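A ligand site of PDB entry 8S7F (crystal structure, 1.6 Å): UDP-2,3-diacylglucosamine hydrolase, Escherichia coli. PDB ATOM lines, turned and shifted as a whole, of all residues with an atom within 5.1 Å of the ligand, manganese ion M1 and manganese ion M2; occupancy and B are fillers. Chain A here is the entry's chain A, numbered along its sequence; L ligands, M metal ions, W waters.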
ATOM      1  N   ASP A   8     -24.375  -9.046 -21.098  1.00  0.00           N
ATOM      2  CA  ASP A   8     -22.935  -9.108 -21.266  1.00  0.00           C
ATOM      3  C   ASP A   8     -22.519  -8.590 -22.644  1.00  0.00           C
ATOM      4  O   ASP A   8     -21.636  -9.157 -23.299  1.00  0.00           O
ATOM      5  CB  ASP A   8     -22.419 -10.519 -20.997  1.00  0.00           C
ATOM      6  CG  ASP A   8     -22.741 -10.948 -19.572  1.00  0.00           C
ATOM      7  OD1 ASP A   8     -22.243 -10.290 -18.639  1.00  0.00           O
ATOM      8  OD2 ASP A   8     -23.523 -11.904 -19.407  1.00  0.00           O
ATOM      9  N   HIS A  10     -21.208  -5.537 -22.762  1.00  0.00           N
ATOM     10  CA  HIS A  10     -19.981  -4.827 -22.400  1.00  0.00           C
ATOM     11  C   HIS A  10     -19.662  -3.742 -23.428  1.00  0.00           C
ATOM     12  O   HIS A  10     -18.513  -3.604 -23.857  1.00  0.00           O
ATOM     13  CB  HIS A  10     -18.819  -5.809 -22.227  1.00  0.00           C
ATOM     14  CG  HIS A  10     -18.918  -6.689 -21.022  1.00  0.00           C
ATOM     15  ND1 HIS A  10     -18.267  -6.379 -19.852  1.00  0.00           N
ATOM     16  CD2 HIS A  10     -19.596  -7.810 -20.791  1.00  0.00           C
ATOM     17  CE1 HIS A  10     -18.536  -7.297 -18.948  1.00  0.00           C
ATOM     18  NE2 HIS A  10     -19.332  -8.185 -19.505  1.00  0.00           N
ATOM     19  N   ASP A  41     -24.556  -5.926 -17.488  1.00  0.00           N
ATOM     20  CA  ASP A  41     -23.328  -5.732 -18.251  1.00  0.00           C
ATOM     21  C   ASP A  41     -23.707  -5.338 -19.677  1.00  0.00           C
ATOM     22  O   ASP A  41     -23.136  -5.844 -20.648  1.00  0.00           O
ATOM     23  CB  ASP A  41     -22.410  -6.960 -18.192  1.00  0.00           C
ATOM     24  CG  ASP A  41     -21.737  -7.242 -16.864  1.00  0.00           C
ATOM     25  OD1 ASP A  41     -21.955  -6.428 -15.893  1.00  0.00           O
ATOM     26  OD2 ASP A  41     -21.014  -8.284 -16.806  1.00  0.00           O
ATOM     27  N   GLU A  44     -19.642  -1.671 -20.489  1.00  0.00           N
ATOM     28  CA  GLU A  44     -18.375  -2.118 -19.917  1.00  0.00           C
ATOM     29  C   GLU A  44     -18.073  -1.404 -18.599  1.00  0.00           C
ATOM     30  O   GLU A  44     -17.293  -1.903 -17.792  1.00  0.00           O
ATOM     31  CB  GLU A  44     -17.250  -1.871 -20.926  1.00  0.00           C
ATOM     32  CG  GLU A  44     -15.855  -2.163 -20.395  1.00  0.00           C
ATOM     33  CD  GLU A  44     -15.622  -3.576 -19.887  1.00  0.00           C
ATOM     34  OE1 GLU A  44     -16.451  -4.458 -20.179  1.00  0.00           O
ATOM     35  OE2 GLU A  44     -14.615  -3.795 -19.184  1.00  0.00           O
ATOM     36  N   ALA A  45     -18.653  -0.213 -18.417  1.00  0.00           N
ATOM     37  CA  ALA A  45     -18.455   0.588 -17.225  1.00  0.00           C
ATOM     38  C   ALA A  45     -19.590   1.590 -17.106  1.00  0.00           C
ATOM     39  O   ALA A  45     -20.234   1.945 -18.098  1.00  0.00           O
ATOM     40  CB  ALA A  45     -17.113   1.286 -17.291  1.00  0.00           C
ATOM     41  N   TRP A  46     -19.840   2.046 -15.871  1.00  0.00           N
ATOM     42  CA  TRP A  46     -20.790   3.115 -15.628  1.00  0.00           C
ATOM     43  C   TRP A  46     -20.382   3.868 -14.370  1.00  0.00           C
ATOM     44  O   TRP A  46     -20.257   3.267 -13.308  1.00  0.00           O
ATOM     45  CB  TRP A  46     -22.211   2.559 -15.496  1.00  0.00           C
ATOM     46  CG  TRP A  46     -23.255   3.587 -15.768  1.00  0.00           C
ATOM     47  CD1 TRP A  46     -23.907   4.394 -14.877  1.00  0.00           C
ATOM     48  CD2 TRP A  46     -23.814   3.884 -17.058  1.00  0.00           C
ATOM     49  NE1 TRP A  46     -24.809   5.188 -15.530  1.00  0.00           N
ATOM     50  CE2 TRP A  46     -24.785   4.886 -16.873  1.00  0.00           C
ATOM     51  CE3 TRP A  46     -23.583   3.381 -18.346  1.00  0.00           C
ATOM     52  CZ2 TRP A  46     -25.535   5.398 -17.932  1.00  0.00           C
ATOM     53  CZ3 TRP A  46     -24.314   3.897 -19.394  1.00  0.00           C
ATOM     54  CH2 TRP A  46     -25.286   4.881 -19.176  1.00  0.00           C
ATOM     55  N   ILE A  47     -20.168   5.176 -14.508  1.00  0.00           N
ATOM     56  CA  ILE A  47     -19.806   5.994 -13.365  1.00  0.00           C
ATOM     57  C   ILE A  47     -20.876   7.056 -13.102  1.00  0.00           C
ATOM     58  O   ILE A  47     -20.658   7.953 -12.286  1.00  0.00           O
ATOM     59  CB  ILE A  47     -18.405   6.627 -13.545  1.00  0.00           C
ATOM     60  CG1 ILE A  47     -18.314   7.490 -14.805  1.00  0.00           C
ATOM     61  CG2 ILE A  47     -17.331   5.556 -13.510  1.00  0.00           C
ATOM     62  CD1 ILE A  47     -17.021   8.254 -14.940  1.00  0.00           C
ATOM     63  N   GLY A  78     -25.664  -5.394 -13.919  1.00  0.00           N
ATOM     64  CA  GLY A  78     -24.522  -6.271 -13.780  1.00  0.00           C
ATOM     65  C   GLY A  78     -23.479  -5.689 -12.839  1.00  0.00           C
ATOM     66  O   GLY A  78     -23.686  -4.643 -12.243  1.00  0.00           O
ATOM     67  N   ASN A  79     -22.336  -6.382 -12.732  1.00  0.00           N
ATOM     68  CA  ASN A  79     -21.238  -5.895 -11.912  1.00  0.00           C
ATOM     69  C   ASN A  79     -20.545  -4.698 -12.562  1.00  0.00           C
ATOM     70  O   ASN A  79     -19.945  -3.898 -11.855  1.00  0.00           O
ATOM     71  CB  ASN A  79     -20.182  -6.951 -11.614  1.00  0.00           C
ATOM     72  CG  ASN A  79     -19.708  -7.647 -12.861  1.00  0.00           C
ATOM     73  OD1 ASN A  79     -20.531  -8.253 -13.538  1.00  0.00           O
ATOM     74  ND2 ASN A  79     -18.422  -7.575 -13.189  1.00  0.00           N
ATOM     75  N   ARG A  80     -20.640  -4.577 -13.897  1.00  0.00           N
ATOM     76  CA  ARG A  80     -20.004  -3.460 -14.570  1.00  0.00           C
ATOM     77  C   ARG A  80     -20.849  -2.197 -14.471  1.00  0.00           C
ATOM     78  O   ARG A  80     -20.284  -1.098 -14.396  1.00  0.00           O
ATOM     79  CB  ARG A  80     -19.715  -3.795 -16.036  1.00  0.00           C
ATOM     80  CG  ARG A  80     -18.869  -5.031 -16.248  1.00  0.00           C
ATOM     81  CD  ARG A  80     -17.531  -5.030 -15.511  1.00  0.00           C
ATOM     82  NE  ARG A  80     -16.697  -3.924 -15.956  1.00  0.00           N
ATOM     83  CZ  ARG A  80     -15.433  -3.739 -15.595  1.00  0.00           C
ATOM     84  NH1 ARG A  80     -14.861  -4.561 -14.735  1.00  0.00           N
ATOM     85  NH2 ARG A  80     -14.752  -2.723 -16.088  1.00  0.00           N
ATOM     86  N   PHE A  82     -23.734  -1.336 -12.401  1.00  0.00           N
ATOM     87  CA  PHE A  82     -24.663  -1.247 -11.271  1.00  0.00           C
ATOM     88  C   PHE A  82     -25.038   0.204 -10.961  1.00  0.00           C
ATOM     89  O   PHE A  82     -26.012   0.418 -10.246  1.00  0.00           O
ATOM     90  CB  PHE A  82     -24.097  -1.949 -10.032  1.00  0.00           C
ATOM     91  CG  PHE A  82     -22.755  -1.435  -9.577  1.00  0.00           C
ATOM     92  CD1 PHE A  82     -22.659  -0.356  -8.706  1.00  0.00           C
ATOM     93  CD2 PHE A  82     -21.588  -1.989 -10.078  1.00  0.00           C
ATOM     94  CE1 PHE A  82     -21.426   0.130  -8.323  1.00  0.00           C
ATOM     95  CE2 PHE A  82     -20.347  -1.483  -9.699  1.00  0.00           C
ATOM     96  CZ  PHE A  82     -20.264  -0.425  -8.815  1.00  0.00           C
ATOM     97  N   LEU A  83     -24.284   1.192 -11.472  1.00  0.00           N
ATOM     98  CA  LEU A  83     -24.607   2.600 -11.231  1.00  0.00           C
ATOM     99  C   LEU A  83     -25.574   3.150 -12.267  1.00  0.00           C
ATOM    100  O   LEU A  83     -25.966   4.322 -12.172  1.00  0.00           O
ATOM    101  CB  LEU A  83     -23.326   3.433 -11.209  1.00  0.00           C
ATOM    102  CG  LEU A  83     -22.433   3.264  -9.978  1.00  0.00           C
ATOM    103  CD1 LEU A  83     -21.297   4.280 -10.022  1.00  0.00           C
ATOM    104  CD2 LEU A  83     -23.236   3.400  -8.692  1.00  0.00           C
ATOM    105  N   HIS A 114     -28.494 -11.222 -13.182  1.00  0.00           N
ATOM    106  CA  HIS A 114     -27.252 -11.098 -13.922  1.00  0.00           C
ATOM    107  C   HIS A 114     -26.441 -12.398 -13.797  1.00  0.00           C
ATOM    108  O   HIS A 114     -25.878 -12.856 -14.790  1.00  0.00           O
ATOM    109  CB  HIS A 114     -26.433  -9.893 -13.449  1.00  0.00           C
ATOM    110  CG  HIS A 114     -25.154  -9.765 -14.189  1.00  0.00           C
ATOM    111  ND1 HIS A 114     -25.148  -9.592 -15.549  1.00  0.00           N
ATOM    112  CD2 HIS A 114     -23.870  -9.782 -13.820  1.00  0.00           C
ATOM    113  CE1 HIS A 114     -23.900  -9.512 -15.971  1.00  0.00           C
ATOM    114  NE2 HIS A 114     -23.110  -9.636 -14.952  1.00  0.00           N
ATOM    115  N   ASP A 122     -16.055 -16.595  -5.331  1.00  0.00           N
ATOM    116  CA  ASP A 122     -15.119 -15.507  -5.549  1.00  0.00           C
ATOM    117  C   ASP A 122     -15.258 -14.508  -4.396  1.00  0.00           C
ATOM    118  O   ASP A 122     -16.061 -13.588  -4.460  1.00  0.00           O
ATOM    119  CB  ASP A 122     -15.289 -14.848  -6.915  1.00  0.00           C
ATOM    120  CG  ASP A 122     -14.190 -13.844  -7.233  1.00  0.00           C
ATOM    121  OD1 ASP A 122     -13.582 -13.310  -6.284  1.00  0.00           O
ATOM    122  OD2 ASP A 122     -13.916 -13.640  -8.421  1.00  0.00           O
ATOM    123  N   GLY A 124     -13.203 -12.236  -3.234  1.00  0.00           N
ATOM    124  CA  GLY A 124     -12.784 -10.889  -3.583  1.00  0.00           C
ATOM    125  C   GLY A 124     -13.877 -10.126  -4.336  1.00  0.00           C
ATOM    126  O   GLY A 124     -14.144  -8.957  -4.045  1.00  0.00           O
ATOM    127  N   TYR A 125     -14.528 -10.809  -5.284  1.00  0.00           N
ATOM    128  CA  TYR A 125     -15.616 -10.168  -6.004  1.00  0.00           C
ATOM    129  C   TYR A 125     -16.789  -9.894  -5.059  1.00  0.00           C
ATOM    130  O   TYR A 125     -17.372  -8.804  -5.107  1.00  0.00           O
ATOM    131  CB  TYR A 125     -16.094 -10.947  -7.237  1.00  0.00           C
ATOM    132  CG  TYR A 125     -17.337 -10.295  -7.767  1.00  0.00           C
ATOM    133  CD1 TYR A 125     -17.292  -9.036  -8.337  1.00  0.00           C
ATOM    134  CD2 TYR A 125     -18.583 -10.847  -7.503  1.00  0.00           C
ATOM    135  CE1 TYR A 125     -18.448  -8.378  -8.728  1.00  0.00           C
ATOM    136  CE2 TYR A 125     -19.745 -10.200  -7.887  1.00  0.00           C
ATOM    137  CZ  TYR A 125     -19.671  -8.967  -8.502  1.00  0.00           C
ATOM    138  OH  TYR A 125     -20.804  -8.308  -8.867  1.00  0.00           O
ATOM    139  N   PHE A 128     -16.228  -6.855  -2.931  1.00  0.00           N
ATOM    140  CA  PHE A 128     -16.404  -5.682  -3.781  1.00  0.00           C
ATOM    141  C   PHE A 128     -17.894  -5.394  -3.968  1.00  0.00           C
ATOM    142  O   PHE A 128     -18.324  -4.258  -3.783  1.00  0.00           O
ATOM    143  CB  PHE A 128     -15.695  -5.884  -5.122  1.00  0.00           C
ATOM    144  CG  PHE A 128     -16.064  -4.901  -6.189  1.00  0.00           C
ATOM    145  CD1 PHE A 128     -17.159  -5.106  -7.016  1.00  0.00           C
ATOM    146  CD2 PHE A 128     -15.318  -3.738  -6.372  1.00  0.00           C
ATOM    147  CE1 PHE A 128     -17.489  -4.191  -7.997  1.00  0.00           C
ATOM    148  CE2 PHE A 128     -15.645  -2.831  -7.363  1.00  0.00           C
ATOM    149  CZ  PHE A 128     -16.735  -3.054  -8.166  1.00  0.00           C
ATOM    150  N   VAL A 132     -19.951  -1.795  -2.964  1.00  0.00           N
ATOM    151  CA  VAL A 132     -20.427  -0.860  -3.973  1.00  0.00           C
ATOM    152  C   VAL A 132     -21.948  -0.901  -4.107  1.00  0.00           C
ATOM    153  O   VAL A 132     -22.509  -0.061  -4.791  1.00  0.00           O
ATOM    154  CB  VAL A 132     -19.738  -1.076  -5.329  1.00  0.00           C
ATOM    155  CG1 VAL A 132     -18.236  -0.892  -5.212  1.00  0.00           C
ATOM    156  CG2 VAL A 132     -20.095  -2.423  -5.949  1.00  0.00           C
ATOM    157  N   LEU A 137     -22.815   4.725  -0.271  1.00  0.00           N
ATOM    158  CA  LEU A 137     -21.528   4.838  -0.950  1.00  0.00           C
ATOM    159  C   LEU A 137     -21.756   5.228  -2.413  1.00  0.00           C
ATOM    160  O   LEU A 137     -20.992   6.025  -2.955  1.00  0.00           O
ATOM    161  CB  LEU A 137     -20.741   3.538  -0.804  1.00  0.00           C
ATOM    162  CG  LEU A 137     -19.361   3.531  -1.477  1.00  0.00           C
ATOM    163  CD1 LEU A 137     -18.462   4.628  -0.910  1.00  0.00           C
ATOM    164  CD2 LEU A 137     -18.689   2.174  -1.327  1.00  0.00           C
ATOM    165  N   GLN A 138     -22.798   4.656  -3.044  1.00  0.00           N
ATOM    166  CA  GLN A 138     -23.141   5.019  -4.405  1.00  0.00           C
ATOM    167  C   GLN A 138     -23.420   6.524  -4.479  1.00  0.00           C
ATOM    168  O   GLN A 138     -22.928   7.207  -5.372  1.00  0.00           O
ATOM    169  CB  GLN A 138     -24.347   4.224  -4.908  1.00  0.00           C
ATOM    170  CG  GLN A 138     -24.053   2.733  -5.036  1.00  0.00           C
ATOM    171  CD  GLN A 138     -25.166   1.968  -5.726  1.00  0.00           C
ATOM    172  OE1 GLN A 138     -26.221   2.518  -6.034  1.00  0.00           O
ATOM    173  NE2 GLN A 138     -24.933   0.690  -5.970  1.00  0.00           N
ATOM    174  N   PHE A 141     -20.169   8.489  -4.133  1.00  0.00           N
ATOM    175  CA  PHE A 141     -19.389   8.381  -5.346  1.00  0.00           C
ATOM    176  C   PHE A 141     -19.946   9.280  -6.458  1.00  0.00           C
ATOM    177  O   PHE A 141     -19.194   9.956  -7.143  1.00  0.00           O
ATOM    178  CB  PHE A 141     -19.361   6.933  -5.836  1.00  0.00           C
ATOM    179  CG  PHE A 141     -18.592   6.738  -7.114  1.00  0.00           C
ATOM    180  CD1 PHE A 141     -17.209   6.687  -7.116  1.00  0.00           C
ATOM    181  CD2 PHE A 141     -19.255   6.660  -8.332  1.00  0.00           C
ATOM    182  CE1 PHE A 141     -16.501   6.511  -8.300  1.00  0.00           C
ATOM    183  CE2 PHE A 141     -18.545   6.493  -9.514  1.00  0.00           C
ATOM    184  CZ  PHE A 141     -17.175   6.408  -9.491  1.00  0.00           C
ATOM    185  N   ILE A 152     -10.869   7.334 -10.838  1.00  0.00           N
ATOM    186  CA  ILE A 152     -11.089   6.188  -9.970  1.00  0.00           C
ATOM    187  C   ILE A 152     -11.383   4.963 -10.842  1.00  0.00           C
ATOM    188  O   ILE A 152     -10.840   3.895 -10.592  1.00  0.00           O
ATOM    189  CB  ILE A 152     -12.205   6.455  -8.944  1.00  0.00           C
ATOM    190  CG1 ILE A 152     -11.807   7.578  -7.974  1.00  0.00           C
ATOM    191  CG2 ILE A 152     -12.588   5.189  -8.205  1.00  0.00           C
ATOM    192  CD1 ILE A 152     -12.935   8.020  -7.062  1.00  0.00           C
ATOM    193  N   ALA A 153     -12.232   5.147 -11.855  1.00  0.00           N
ATOM    194  CA  ALA A 153     -12.685   4.058 -12.712  1.00  0.00           C
ATOM    195  C   ALA A 153     -11.498   3.441 -13.445  1.00  0.00           C
ATOM    196  O   ALA A 153     -11.344   2.212 -13.447  1.00  0.00           O
ATOM    197  CB  ALA A 153     -13.715   4.553 -13.688  1.00  0.00           C
ATOM    198  N   MET A 156      -9.613   1.295 -11.181  1.00  0.00           N
ATOM    199  CA  MET A 156     -10.406   0.162 -10.738  1.00  0.00           C
ATOM    200  C   MET A 156     -10.571  -0.856 -11.870  1.00  0.00           C
ATOM    201  O   MET A 156     -10.606  -2.063 -11.618  1.00  0.00           O
ATOM    202  CB  MET A 156     -11.785   0.608 -10.254  1.00  0.00           C
ATOM    203  CG  MET A 156     -11.859   0.702  -8.746  1.00  0.00           C
ATOM    204  SD  MET A 156     -13.286   1.644  -8.177  1.00  0.00           S
ATOM    205  CE  MET A 156     -12.762   2.045  -6.516  1.00  0.00           C
ATOM    206  N   ARG A 157     -10.672  -0.362 -13.109  1.00  0.00           N
ATOM    207  CA  ARG A 157     -10.782  -1.224 -14.279  1.00  0.00           C
ATOM    208  C   ARG A 157      -9.438  -1.906 -14.533  1.00  0.00           C
ATOM    209  O   ARG A 157      -9.401  -3.086 -14.885  1.00  0.00           O
ATOM    210  CB  ARG A 157     -11.262  -0.409 -15.485  1.00  0.00           C
ATOM    211  CG  ARG A 157     -12.693   0.088 -15.359  1.00  0.00           C
ATOM    212  CD  ARG A 157     -13.084   1.060 -16.453  1.00  0.00           C
ATOM    213  NE  ARG A 157     -13.092   0.447 -17.775  1.00  0.00           N
ATOM    214  CZ  ARG A 157     -13.398   1.090 -18.896  1.00  0.00           C
ATOM    215  NH1 ARG A 157     -13.764   2.364 -18.854  1.00  0.00           N
ATOM    216  NH2 ARG A 157     -13.350   0.461 -20.055  1.00  0.00           N
ATOM    217  N   ALA A 170     -10.149 -13.410 -15.686  1.00  0.00           N
ATOM    218  CA  ALA A 170     -11.044 -14.589 -15.645  1.00  0.00           C
ATOM    219  C   ALA A 170     -12.203 -14.339 -14.695  1.00  0.00           C
ATOM    220  O   ALA A 170     -12.005 -13.829 -13.589  1.00  0.00           O
ATOM    221  CB  ALA A 170     -10.240 -15.807 -15.241  1.00  0.00           C
ATOM    222  N   ILE A 171     -13.416 -14.701 -15.131  1.00  0.00           N
ATOM    223  CA  ILE A 171     -14.625 -14.553 -14.333  1.00  0.00           C
ATOM    224  C   ILE A 171     -14.935 -15.909 -13.704  1.00  0.00           C
ATOM    225  O   ILE A 171     -15.080 -16.896 -14.404  1.00  0.00           O
ATOM    226  CB  ILE A 171     -15.787 -14.052 -15.201  1.00  0.00           C
ATOM    227  CG1 ILE A 171     -15.461 -12.720 -15.870  1.00  0.00           C
ATOM    228  CG2 ILE A 171     -17.083 -13.986 -14.396  1.00  0.00           C
ATOM    229  CD1 ILE A 171     -16.375 -12.357 -17.029  1.00  0.00           C
ATOM    230  N   HIS A 195     -23.330 -13.105 -16.939  1.00  0.00           N
ATOM    231  CA  HIS A 195     -22.181 -12.835 -16.069  1.00  0.00           C
ATOM    232  C   HIS A 195     -20.988 -13.761 -16.331  1.00  0.00           C
ATOM    233  O   HIS A 195     -19.861 -13.268 -16.440  1.00  0.00           O
ATOM    234  CB  HIS A 195     -22.533 -12.888 -14.588  1.00  0.00           C
ATOM    235  CG  HIS A 195     -21.349 -12.577 -13.738  1.00  0.00           C
ATOM    236  ND1 HIS A 195     -20.716 -11.347 -13.733  1.00  0.00           N
ATOM    237  CD2 HIS A 195     -20.675 -13.369 -12.894  1.00  0.00           C
ATOM    238  CE1 HIS A 195     -19.701 -11.414 -12.886  1.00  0.00           C
ATOM    239  NE2 HIS A 195     -19.657 -12.625 -12.361  1.00  0.00           N
ATOM    240  N   HIS A 197     -20.087 -15.657 -18.816  1.00  0.00           N
ATOM    241  CA  HIS A 197     -19.550 -15.704 -20.173  1.00  0.00           C
ATOM    242  C   HIS A 197     -19.324 -17.148 -20.633  1.00  0.00           C
ATOM    243  O   HIS A 197     -18.429 -17.424 -21.430  1.00  0.00           O
ATOM    244  CB  HIS A 197     -18.309 -14.824 -20.324  1.00  0.00           C
ATOM    245  CG  HIS A 197     -18.532 -13.386 -20.016  1.00  0.00           C
ATOM    246  ND1 HIS A 197     -17.520 -12.461 -20.161  1.00  0.00           N
ATOM    247  CD2 HIS A 197     -19.598 -12.688 -19.576  1.00  0.00           C
ATOM    248  CE1 HIS A 197     -17.974 -11.260 -19.841  1.00  0.00           C
ATOM    249  NE2 HIS A 197     -19.232 -11.366 -19.476  1.00  0.00           N
HETATM  250  C1  LIG L   1     -18.736   3.026  -5.946  1.00  0.00           C
HETATM  251  C2  LIG L   1     -17.710   3.573  -5.198  1.00  0.00           C
HETATM  252  C3  LIG L   1     -18.349   2.444 -10.148  1.00  0.00           C
HETATM  253  C4  LIG L   1     -16.006   2.851  -9.951  1.00  0.00           C
HETATM  254  C5  LIG L   1     -16.504   3.726  -5.862  1.00  0.00           C
HETATM  255  C6  LIG L   1     -16.318   3.350  -7.172  1.00  0.00           C
HETATM  256  C7  LIG L   1     -17.373   2.824  -7.901  1.00  0.00           C
HETATM  257  C8  LIG L   1     -18.095   1.402 -11.235  1.00  0.00           C
HETATM  258  C9  LIG L   1     -18.594   2.657  -7.260  1.00  0.00           C
HETATM  259  N1  LIG L   1     -17.204   2.415  -9.239  1.00  0.00           N
HETATM  260  C10 LIG L   1     -15.687   1.793 -11.012  1.00  0.00           C
HETATM  261  N2  LIG L   1     -16.823   1.704 -11.956  1.00  0.00           N
HETATM  262  S1  LIG L   1     -16.545   0.797 -13.282  1.00  0.00           S
HETATM  263  C11 LIG L   1     -16.173  -0.806 -12.678  1.00  0.00           C
HETATM  264  O1  LIG L   1     -17.783   0.775 -13.996  1.00  0.00           O
HETATM  265  O2  LIG L   1     -15.368   1.322 -13.913  1.00  0.00           O
HETATM  266  C12 LIG L   1     -14.853  -1.092 -12.383  1.00  0.00           C
HETATM  267  C13 LIG L   1     -14.516  -2.323 -11.880  1.00  0.00           C
HETATM  268  C14 LIG L   1     -15.464  -3.309 -11.691  1.00  0.00           C
HETATM  269  C15 LIG L   1     -17.156  -1.772 -12.461  1.00  0.00           C
HETATM  270  C16 LIG L   1     -16.803  -3.018 -11.950  1.00  0.00           C
HETATM  271  N3  LIG L   1     -15.019  -4.499 -11.127  1.00  0.00           N
HETATM  272  C17 LIG L   1     -15.681  -5.688 -11.061  1.00  0.00           C
HETATM  273  O3  LIG L   1     -16.782  -5.844 -11.565  1.00  0.00           O
HETATM  274  C18 LIG L   1     -14.973  -6.786 -10.309  1.00  0.00           C
HETATM  275  C19 LIG L   1     -14.485  -6.442  -9.046  1.00  0.00           C
HETATM  276  C20 LIG L   1     -13.801  -7.362  -8.284  1.00  0.00           C
HETATM  277  C21 LIG L   1     -13.610  -8.650  -8.769  1.00  0.00           C
HETATM  278  C22 LIG L   1     -14.104  -8.995 -10.024  1.00  0.00           C
HETATM  279  C23 LIG L   1     -14.781  -8.065 -10.791  1.00  0.00           C
HETATM  280  N4  LIG L   1     -15.296  -8.425 -12.098  1.00  0.00           N
HETATM  281  C24 LIG L   1     -16.001  -9.726 -12.240  1.00  0.00           C
HETATM  282  S2  LIG L   1     -14.417  -7.958 -13.395  1.00  0.00           S
HETATM  283  C25 LIG L   1     -13.057  -9.094 -13.536  1.00  0.00           C
HETATM  284  O4  LIG L   1     -15.233  -8.086 -14.560  1.00  0.00           O
HETATM  285  O5  LIG L   1     -13.850  -6.675 -13.128  1.00  0.00           O
HETATM  286 CL1  LIG L   1     -20.284   2.823  -5.194  1.00  0.00          CL
HETATM  287 CL2  LIG L   1     -15.154   4.424  -4.998  1.00  0.00          CL
HETATM  288 MN    MN M   1     -20.934  -9.595 -15.122  1.00  0.00          MN
HETATM  289 MN    MN M   2     -20.241  -9.772 -18.332  1.00  0.00          MN
HETATM  290  O   HOH W   1     -17.678  -8.874 -15.679  1.00  0.00           O
HETATM  291  O   HOH W   2     -12.242  -4.333 -10.279  1.00  0.00           O
HETATM  292  O   HOH W   3     -19.593 -10.577 -16.486  1.00  0.00           O
HETATM  293  O   HOH W   4     -13.164 -11.865 -12.061  1.00  0.00           O
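Within 4 Å of manganese ion M2: Asp 8, His 10, Asp 41, His 195 and His 197.
The nearest printed residue that does not touch manganese ion M2 is His 114 (4.4 Å).
Water W1 lies within hydrogen-bond range of O4 of the ligand and ND2 of Asn 79.
Water W2 lies within hydrogen-bond range of a nitrogen (N3) of the ligand (2.9 Å) and the backbone carbonyl oxygen of Met 156 (3.1 Å).
OD1 of Asn 79 is bound to manganese ion M1 (2.1 Å).
The side-chain carboxylate (OD2) of Asp 41 binds manganese ion M1 (2.1 Å).
Manganese ion M1 is bound by water W3 (2.2 Å).
A ring nitrogen (NE2) of His 114 binds manganese ion M1, at 2.2 Å.
ND1 of His 195 binds manganese ion M1, 2.2 Å away.
Merely in contact with the ligand: Ala 45 (3.3 Å), Phe 82 (3.7 Å), Leu 83 (3.5 Å), Tyr 125 (3.6 Å), Phe 128 (3.6 Å), Val 132 (3.7 Å), Leu 137 (3.9 Å), Gln 138 (3.7 Å), Phe 141 (3.3 Å), Ala 153 (3.6 Å), Met 156 (3.5 Å) and Arg 157 (3.3 Å).
Hydrophobic or aromatic side chains that line the ligand: Ala 45, Phe 82, Leu 83, Tyr 125, Phe 128, Val 132, Leu 137, Phe 141, Ala 153 and Met 156.
Of the 29 residues printed, 15 come within 4 Å of the ligand.
A ring nitrogen (ND1) of His 10 lies within hydrogen-bond range of the side-chain carboxylate (OE1) of Glu 44 (2.7 Å).
O of Val 132 is in hydrogen-bond range of NE2 of Gln 138 (2.8 Å).
The side-chain carboxylate (OD2) of Asp 8 sits at hydrogen-bond distance from the backbone NH (N) of His 195 (2.8 Å).
OD1 of Asp 122 sits at hydrogen-bond distance from N of Tyr 125 (2.9 Å).
OE2 of Glu 44 lies within salt-bridge range of NH2 of Arg 80.
The side-chain carboxylate (OD1) of Asp 41 lies within hydrogen-bond range of the backbone NH (N) of Arg 80, 3.0 Å away.
Of the 29 residues printed, 5 come within 4 Å of manganese ion M1.
The guanidinium group of Arg 80 sits at hydrogen-bond distance from an oxygen (O5) of the ligand, at 2.8 Å.
The backbone NH (N) of Trp 46 lies within hydrogen-bond range of an oxygen (O1) of the ligand (3.1 Å).
The side-chain amide nitrogen (ND2) of Asn 79 sits at hydrogen-bond distance from an oxygen (O3) of the ligand, at 2.9 Å.
Manganese ion M2 is bound by the side-chain carboxylate of Asp 8, water W3, a ring nitrogen (NE2) of His 10, a ring nitrogen (NE2) of His 197 and the side-chain carboxylate of Asp 41.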
